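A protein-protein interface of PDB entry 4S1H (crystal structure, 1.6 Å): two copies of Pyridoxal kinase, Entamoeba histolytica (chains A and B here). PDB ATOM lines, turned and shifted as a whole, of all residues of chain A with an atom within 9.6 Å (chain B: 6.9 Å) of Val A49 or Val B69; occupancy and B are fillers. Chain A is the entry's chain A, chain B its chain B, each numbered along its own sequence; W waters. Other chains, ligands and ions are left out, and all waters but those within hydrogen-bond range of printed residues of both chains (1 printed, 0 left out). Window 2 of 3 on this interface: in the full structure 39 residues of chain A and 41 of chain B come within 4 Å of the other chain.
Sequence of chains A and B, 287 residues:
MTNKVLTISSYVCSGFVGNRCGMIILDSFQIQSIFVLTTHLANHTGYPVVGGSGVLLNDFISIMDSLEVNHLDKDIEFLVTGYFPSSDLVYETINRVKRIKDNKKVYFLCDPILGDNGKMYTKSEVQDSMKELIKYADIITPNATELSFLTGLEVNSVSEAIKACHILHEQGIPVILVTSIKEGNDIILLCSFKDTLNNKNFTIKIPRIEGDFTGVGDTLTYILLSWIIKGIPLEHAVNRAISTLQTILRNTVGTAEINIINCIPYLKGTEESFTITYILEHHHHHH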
ATOM      1  N   VAL A  12     -23.204  16.374  21.753  1.00  0.00           N
ATOM      2  CA  VAL A  12     -23.059  15.514  22.938  1.00  0.00           C
ATOM      3  C   VAL A  12     -23.004  16.357  24.206  1.00  0.00           C
ATOM      4  O   VAL A  12     -22.356  17.402  24.216  1.00  0.00           O
ATOM      5  CB  VAL A  12     -21.796  14.614  22.888  1.00  0.00           C
ATOM      6  CG1 VAL A  12     -22.005  13.559  21.828  1.00  0.00           C
ATOM      7  CG2 VAL A  12     -20.520  15.431  22.612  1.00  0.00           C
ATOM      8  N   LEU A  41     -27.302  13.829  22.241  1.00  0.00           N
ATOM      9  CA  LEU A  41     -26.864  12.598  22.882  1.00  0.00           C
ATOM     10  C   LEU A  41     -26.116  12.890  24.168  1.00  0.00           C
ATOM     11  O   LEU A  41     -25.514  13.942  24.313  1.00  0.00           O
ATOM     12  CB  LEU A  41     -25.906  11.834  21.973  1.00  0.00           C
ATOM     13  CG  LEU A  41     -26.426  11.631  20.547  1.00  0.00           C
ATOM     14  CD1 LEU A  41     -25.366  10.942  19.711  1.00  0.00           C
ATOM     15  CD2 LEU A  41     -27.702  10.816  20.560  1.00  0.00           C
ATOM     16  N   ALA A  42     -26.125  11.944  25.081  1.00  0.00           N
ATOM     17  CA  ALA A  42     -25.392  12.084  26.338  1.00  0.00           C
ATOM     18  C   ALA A  42     -23.900  12.162  26.124  1.00  0.00           C
ATOM     19  O   ALA A  42     -23.204  12.915  26.767  1.00  0.00           O
ATOM     20  CB  ALA A  42     -25.689  10.910  27.242  1.00  0.00           C
ATOM     21  N   ASN A  43     -23.419  11.308  25.207  1.00  0.00           N
ATOM     22  CA  ASN A  43     -21.990  11.125  24.981  1.00  0.00           C
ATOM     23  C   ASN A  43     -21.796  10.538  23.575  1.00  0.00           C
ATOM     24  O   ASN A  43     -22.766  10.218  22.905  1.00  0.00           O
ATOM     25  CB  ASN A  43     -21.409  10.213  26.064  1.00  0.00           C
ATOM     26  CG  ASN A  43     -22.273   8.989  26.339  1.00  0.00           C
ATOM     27  OD1 ASN A  43     -22.967   8.905  27.360  1.00  0.00           O
ATOM     28  ND2 ASN A  43     -22.257   8.032  25.399  1.00  0.00           N
ATOM     29  N   HIS A  44     -20.564  10.453  23.105  1.00  0.00           N
ATOM     30  CA  HIS A  44     -20.374   9.973  21.742  1.00  0.00           C
ATOM     31  C   HIS A  44     -20.585   8.455  21.607  1.00  0.00           C
ATOM     32  O   HIS A  44     -20.745   7.734  22.593  1.00  0.00           O
ATOM     33  CB  HIS A  44     -19.071  10.489  21.121  1.00  0.00           C
ATOM     34  CG  HIS A  44     -17.837   9.991  21.784  1.00  0.00           C
ATOM     35  ND1 HIS A  44     -17.511   8.651  21.857  1.00  0.00           N
ATOM     36  CD2 HIS A  44     -16.803  10.658  22.338  1.00  0.00           C
ATOM     37  CE1 HIS A  44     -16.357   8.514  22.470  1.00  0.00           C
ATOM     38  NE2 HIS A  44     -15.900   9.715  22.766  1.00  0.00           N
ATOM     39  N   THR A  45     -20.622   8.002  20.353  1.00  0.00           N
ATOM     40  CA  THR A  45     -21.028   6.631  19.996  1.00  0.00           C
ATOM     41  C   THR A  45     -20.002   5.547  20.386  1.00  0.00           C
ATOM     42  O   THR A  45     -20.302   4.347  20.396  1.00  0.00           O
ATOM     43  CB  THR A  45     -21.400   6.585  18.495  1.00  0.00           C
ATOM     44  OG1 THR A  45     -20.364   7.209  17.733  1.00  0.00           O
ATOM     45  CG2 THR A  45     -22.680   7.377  18.226  1.00  0.00           C
ATOM     46  N   GLY A  46     -18.781   5.975  20.677  1.00  0.00           N
ATOM     47  CA  GLY A  46     -17.757   5.139  21.321  1.00  0.00           C
ATOM     48  C   GLY A  46     -18.042   4.472  22.663  1.00  0.00           C
ATOM     49  O   GLY A  46     -17.392   3.486  23.007  1.00  0.00           O
ATOM     50  N   TYR A  47     -18.989   4.998  23.441  1.00  0.00           N
ATOM     51  CA  TYR A  47     -19.319   4.414  24.729  1.00  0.00           C
ATOM     52  C   TYR A  47     -20.327   3.259  24.568  1.00  0.00           C
ATOM     53  O   TYR A  47     -21.050   3.225  23.559  1.00  0.00           O
ATOM     54  CB  TYR A  47     -19.908   5.488  25.671  1.00  0.00           C
ATOM     55  CG  TYR A  47     -18.909   6.586  26.043  1.00  0.00           C
ATOM     56  CD1 TYR A  47     -18.706   7.693  25.209  1.00  0.00           C
ATOM     57  CD2 TYR A  47     -18.162   6.498  27.196  1.00  0.00           C
ATOM     58  CE1 TYR A  47     -17.801   8.700  25.533  1.00  0.00           C
ATOM     59  CE2 TYR A  47     -17.244   7.496  27.526  1.00  0.00           C
ATOM     60  CZ  TYR A  47     -17.075   8.587  26.701  1.00  0.00           C
ATOM     61  OH  TYR A  47     -16.138   9.563  27.002  1.00  0.00           O
ATOM     62  N   PRO A  48     -20.407   2.351  25.555  1.00  0.00           N
ATOM     63  CA  PRO A  48     -21.365   1.228  25.551  1.00  0.00           C
ATOM     64  C   PRO A  48     -22.844   1.591  25.524  1.00  0.00           C
ATOM     65  O   PRO A  48     -23.650   0.804  25.052  1.00  0.00           O
ATOM     66  CB  PRO A  48     -21.087   0.504  26.867  1.00  0.00           C
ATOM     67  CG  PRO A  48     -19.738   0.927  27.280  1.00  0.00           C
ATOM     68  CD  PRO A  48     -19.485   2.273  26.706  1.00  0.00           C
ATOM     69  N   VAL A  49     -23.200   2.735  26.101  1.00  0.00           N
ATOM     70  CA  VAL A  49     -24.571   3.211  26.094  1.00  0.00           C
ATOM     71  C   VAL A  49     -24.485   4.622  25.553  1.00  0.00           C
ATOM     72  O   VAL A  49     -23.550   5.340  25.895  1.00  0.00           O
ATOM     73  CB  VAL A  49     -25.128   3.196  27.532  1.00  0.00           C
ATOM     74  CG1 VAL A  49     -26.512   3.818  27.624  1.00  0.00           C
ATOM     75  CG2 VAL A  49     -25.164   1.781  28.094  1.00  0.00           C
ATOM     76  N   VAL A  50     -25.408   4.971  24.654  1.00  0.00           N
ATOM     77  CA  VAL A  50     -25.477   6.289  24.040  1.00  0.00           C
ATOM     78  C   VAL A  50     -26.912   6.796  24.170  1.00  0.00           C
ATOM     79  O   VAL A  50     -27.740   6.593  23.296  1.00  0.00           O
ATOM     80  CB  VAL A  50     -25.054   6.278  22.556  1.00  0.00           C
ATOM     81  CG1 VAL A  50     -24.939   7.685  22.000  1.00  0.00           C
ATOM     82  CG2 VAL A  50     -23.719   5.549  22.380  1.00  0.00           C
ATOM     83  N   GLY A  51     -27.199   7.518  25.250  1.00  0.00           N
ATOM     84  CA  GLY A  51     -28.562   7.962  25.490  1.00  0.00           C
ATOM     85  C   GLY A  51     -28.885   9.192  24.651  1.00  0.00           C
ATOM     86  O   GLY A  51     -27.993   9.912  24.214  1.00  0.00           O
ATOM     87  N   GLY A  52     -30.165   9.386  24.385  1.00  0.00           N
ATOM     88  CA  GLY A  52     -30.674  10.535  23.640  1.00  0.00           C
ATOM     89  C   GLY A  52     -31.051  10.163  22.209  1.00  0.00           C
ATOM     90  O   GLY A  52     -30.927   8.999  21.812  1.00  0.00           O
ATOM     91  N   SER B  62     -33.141   9.102  29.129  1.00  0.00           N
ATOM     92  CA  SER B  62     -32.168   8.316  28.397  1.00  0.00           C
ATOM     93  C   SER B  62     -30.765   8.924  28.554  1.00  0.00           C
ATOM     94  O   SER B  62     -29.777   8.211  28.743  1.00  0.00           O
ATOM     95  CB  SER B  62     -32.548   8.307  26.923  1.00  0.00           C
ATOM     96  OG  SER B  62     -31.660   7.514  26.189  1.00  0.00           O
ATOM     97  N   MET B  64     -29.737  11.078  30.988  1.00  0.00           N
ATOM     98  CA  MET B  64     -29.251  11.018  32.359  1.00  0.00           C
ATOM     99  C   MET B  64     -28.788   9.609  32.717  1.00  0.00           C
ATOM    100  O   MET B  64     -27.748   9.432  33.395  1.00  0.00           O
ATOM    101  CB  MET B  64     -30.305  11.521  33.357  1.00  0.00           C
ATOM    102  CG  MET B  64     -30.623  12.995  33.159  1.00  0.00           C
ATOM    103  SD  MET B  64     -29.260  14.136  33.400  1.00  0.00           S
ATOM    104  CE  MET B  64     -29.055  13.987  35.184  1.00  0.00           C
ATOM    105  N   ASP B  65     -29.531   8.600  32.262  1.00  0.00           N
ATOM    106  CA  ASP B  65     -29.144   7.206  32.482  1.00  0.00           C
ATOM    107  C   ASP B  65     -27.810   6.891  31.845  1.00  0.00           C
ATOM    108  O   ASP B  65     -26.995   6.223  32.445  1.00  0.00           O
ATOM    109  CB  ASP B  65     -30.181   6.235  31.915  1.00  0.00           C
ATOM    110  CG  ASP B  65     -31.457   6.169  32.735  1.00  0.00           C
ATOM    111  OD1 ASP B  65     -31.532   6.732  33.861  1.00  0.00           O
ATOM    112  OD2 ASP B  65     -32.419   5.544  32.230  1.00  0.00           O
ATOM    113  N   SER B  66     -27.607   7.369  30.621  1.00  0.00           N
ATOM    114  CA  SER B  66     -26.369   7.141  29.910  1.00  0.00           C
ATOM    115  C   SER B  66     -25.155   7.780  30.606  1.00  0.00           C
ATOM    116  O   SER B  66     -24.099   7.146  30.729  1.00  0.00           O
ATOM    117  CB  SER B  66     -26.532   7.687  28.504  1.00  0.00           C
ATOM    118  OG  SER B  66     -25.421   7.469  27.695  1.00  0.00           O
ATOM    119  N   LEU B  67     -25.303   9.011  31.077  1.00  0.00           N
ATOM    120  CA  LEU B  67     -24.251   9.652  31.878  1.00  0.00           C
ATOM    121  C   LEU B  67     -23.892   8.865  33.119  1.00  0.00           C
ATOM    122  O   LEU B  67     -22.730   8.694  33.416  1.00  0.00           O
ATOM    123  CB  LEU B  67     -24.648  11.048  32.301  1.00  0.00           C
ATOM    124  CG  LEU B  67     -24.865  12.002  31.130  1.00  0.00           C
ATOM    125  CD1 LEU B  67     -25.513  13.263  31.621  1.00  0.00           C
ATOM    126  CD2 LEU B  67     -23.589  12.347  30.381  1.00  0.00           C
ATOM    127  N   GLU B  68     -24.897   8.345  33.817  1.00  0.00           N
ATOM    128  CA  GLU B  68     -24.674   7.526  35.013  1.00  0.00           C
ATOM    129  C   GLU B  68     -23.968   6.200  34.695  1.00  0.00           C
ATOM    130  O   GLU B  68     -22.946   5.871  35.303  1.00  0.00           O
ATOM    131  CB  GLU B  68     -25.991   7.259  35.757  1.00  0.00           C
ATOM    132  CG  GLU B  68     -25.798   6.663  37.150  1.00  0.00           C
ATOM    133  CD  GLU B  68     -27.102   6.453  37.901  1.00  0.00           C
ATOM    134  OE1 GLU B  68     -27.956   7.361  37.860  1.00  0.00           O
ATOM    135  OE2 GLU B  68     -27.272   5.387  38.537  1.00  0.00           O
ATOM    136  N   VAL B  69     -24.504   5.446  33.737  1.00  0.00           N
ATOM    137  CA  VAL B  69     -23.995   4.113  33.407  1.00  0.00           C
ATOM    138  C   VAL B  69     -22.560   4.175  32.897  1.00  0.00           C
ATOM    139  O   VAL B  69     -21.753   3.280  33.186  1.00  0.00           O
ATOM    140  CB  VAL B  69     -24.895   3.403  32.361  1.00  0.00           C
ATOM    141  CG1 VAL B  69     -24.221   2.165  31.747  1.00  0.00           C
ATOM    142  CG2 VAL B  69     -26.205   3.004  33.019  1.00  0.00           C
ATOM    143  N   ASN B  70     -22.258   5.196  32.094  1.00  0.00           N
ATOM    144  CA  ASN B  70     -20.901   5.406  31.609  1.00  0.00           C
ATOM    145  C   ASN B  70     -19.943   6.106  32.589  1.00  0.00           C
ATOM    146  O   ASN B  70     -18.802   6.411  32.212  1.00  0.00           O
ATOM    147  CB  ASN B  70     -20.929   6.158  30.275  1.00  0.00           C
ATOM    148  CG  ASN B  70     -21.575   5.355  29.158  1.00  0.00           C
ATOM    149  OD1 ASN B  70     -21.318   4.153  28.998  1.00  0.00           O
ATOM    150  ND2 ASN B  70     -22.356   6.039  28.323  1.00  0.00           N
ATOM    151  N   HIS B  71     -20.407   6.350  33.821  1.00  0.00           N
ATOM    152  CA  HIS B  71     -19.627   6.952  34.894  1.00  0.00           C
ATOM    153  C   HIS B  71     -19.103   8.357  34.597  1.00  0.00           C
ATOM    154  O   HIS B  71     -18.077   8.767  35.134  1.00  0.00           O
ATOM    155  CB  HIS B  71     -18.510   6.003  35.330  1.00  0.00           C
ATOM    156  CG  HIS B  71     -18.991   4.603  35.531  1.00  0.00           C
ATOM    157  ND1 HIS B  71     -19.748   4.222  36.620  1.00  0.00           N
ATOM    158  CD2 HIS B  71     -18.869   3.499  34.754  1.00  0.00           C
ATOM    159  CE1 HIS B  71     -20.047   2.938  36.520  1.00  0.00           C
ATOM    160  NE2 HIS B  71     -19.529   2.478  35.396  1.00  0.00           N
ATOM    161  N   LEU B  72     -19.826   9.079  33.752  1.00  0.00           N
ATOM    162  CA  LEU B  72     -19.429  10.419  33.316  1.00  0.00           C
ATOM    163  C   LEU B  72     -19.822  11.500  34.302  1.00  0.00           C
ATOM    164  O   LEU B  72     -19.279  12.600  34.223  1.00  0.00           O
ATOM    165  CB  LEU B  72     -20.011  10.704  31.930  1.00  0.00           C
ATOM    166  CG  LEU B  72     -19.510   9.762  30.831  1.00  0.00           C
ATOM    167  CD1 LEU B  72     -20.261   9.928  29.518  1.00  0.00           C
ATOM    168  CD2 LEU B  72     -18.019   9.934  30.602  1.00  0.00           C
ATOM    169  N   ASP B  73     -20.701  11.162  35.250  1.00  0.00           N
ATOM    170  CA  ASP B  73     -21.150  12.080  36.287  1.00  0.00           C
ATOM    171  C   ASP B  73     -20.702  11.695  37.703  1.00  0.00           C
ATOM    172  O   ASP B  73     -21.225  12.253  38.688  1.00  0.00           O
ATOM    173  CB  ASP B  73     -22.686  12.198  36.265  1.00  0.00           C
ATOM    174  CG  ASP B  73     -23.411  10.895  36.660  1.00  0.00           C
ATOM    175  OD1 ASP B  73     -22.766   9.819  36.773  1.00  0.00           O
ATOM    176  OD2 ASP B  73     -24.647  10.945  36.811  1.00  0.00           O
HETATM  177  O   HOH W   1     -33.646   8.559  23.814  1.00  0.00           O
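The side-chain hydroxyl (OG) of Ser B66 lies within hydrogen-bond range of the side-chain amide oxygen (OD1) of Asn A43, at 2.9 Å. The side-chain amide nitrogen (ND2) of Asn B70 is in hydrogen-bond range of the side-chain amide oxygen (OD1) of Asn A43 (3.1 Å). The backbone carbonyl oxygen (O) of Val A49 is in hydrogen-bond range of the side-chain hydroxyl (OG) of Ser B66 (3.4 Å). O of Val A49 is in hydrogen-bond range of ND2 of Asn B70 (2.8 Å). OG of Ser B66 lies within hydrogen-bond range of N of Gly A51, at 3.0 Å. N of Gly A52 is in hydrogen-bond range of OG of Ser B62.
The backbone NH (N) of Ala A42 lies within hydrogen-bond range of the backbone carbonyl oxygen (O) of Gly A51 (2.9 Å). O of Val A49 sits at hydrogen-bond distance from ND2 of Asn A43 (3.0 Å). The side-chain amide nitrogen (ND2) of Asn B70 sits at hydrogen-bond distance from the backbone carbonyl oxygen (O) of Ser B66, 3.2 Å away. N of Leu B72 sits at hydrogen-bond distance from O of Leu B67. NE2 of His B71 lies within hydrogen-bond range of O of Val B69 (3.2 Å).
Among the printed residues, merely in contact across the chains: Ala A42 with Ser B66 (3.5 Å), Ala A42 with Leu B67 (3.7 Å), Asn A43 with Leu B72 (3.6 Å), Tyr A47 with Asn B70 (3.7 Å), Pro A48 with Asn B70 (3.5 Å), Val A49 with Val B69 (3.8 Å), Val A50 with Ser B66 (3.8 Å) and Gly A51 with Ser B62 (3.2 Å).
Val B69 touches just one residue of chain A: Val A49 (3.8 Å). Asn B70 touches just these residues of chain A: Asn A43, Tyr A47, Pro A48 and Val A49. Of the printed residues of chain B, Gly A51 touches Ser B62 (3.2 Å) and Ser B66 (3.0 Å). Printed residues of chain B within 4 Å of Asn A43: Ser B66 (2.9 Å), Asn B70 (3.1 Å) and Leu B72 (3.6 Å). Of the printed residues of chain A, Leu B72 touches Asn A43. Of the printed residues of chain B, Gly A52 touches Ser B62. Of the printed residues of chain A, Leu B67 touches Ala A42. The nearest residue of chain A that does not touch Val B69 is Pro A48 (6.0 Å). The nearest printed residue of chain B that does not touch Tyr A47 is Leu B72 (4.001 Å).
Of the 11 printed residues of chain B, 6 touch a printed residue of chain A. Printed residues of chain B that touch a printed residue of chain A: Ser B62, Ser B66, Leu B67, Val B69, Asn B70 and Leu B72. Hydrophobic or aromatic side chains of chain B within 4 Å of the printed part of chain A: Leu B67, Val B69 and Leu B72. Of the 13 printed residues of chain A, 8 touch a printed residue of chain B. Hydrophobic or aromatic side chains of chain A that line the printed part of chain B: Ala A42, Tyr A47, Pro A48 and Val A49. Among the printed residues, 14 pairs touch across the chains. Among the printed residues, no Asp or Glu carboxylate lies within 4 Å of a Lys or Arg side-chain nitrogen of the other chain.
No position is printed for both chains. Of the 14 pairs that touch across the chains among the printed residues, none has its exchanged pair printed and touching as well.
Water W1 bridges OG of Ser B62 (3.3 Å) and O of Gly A52 (3.4 Å).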
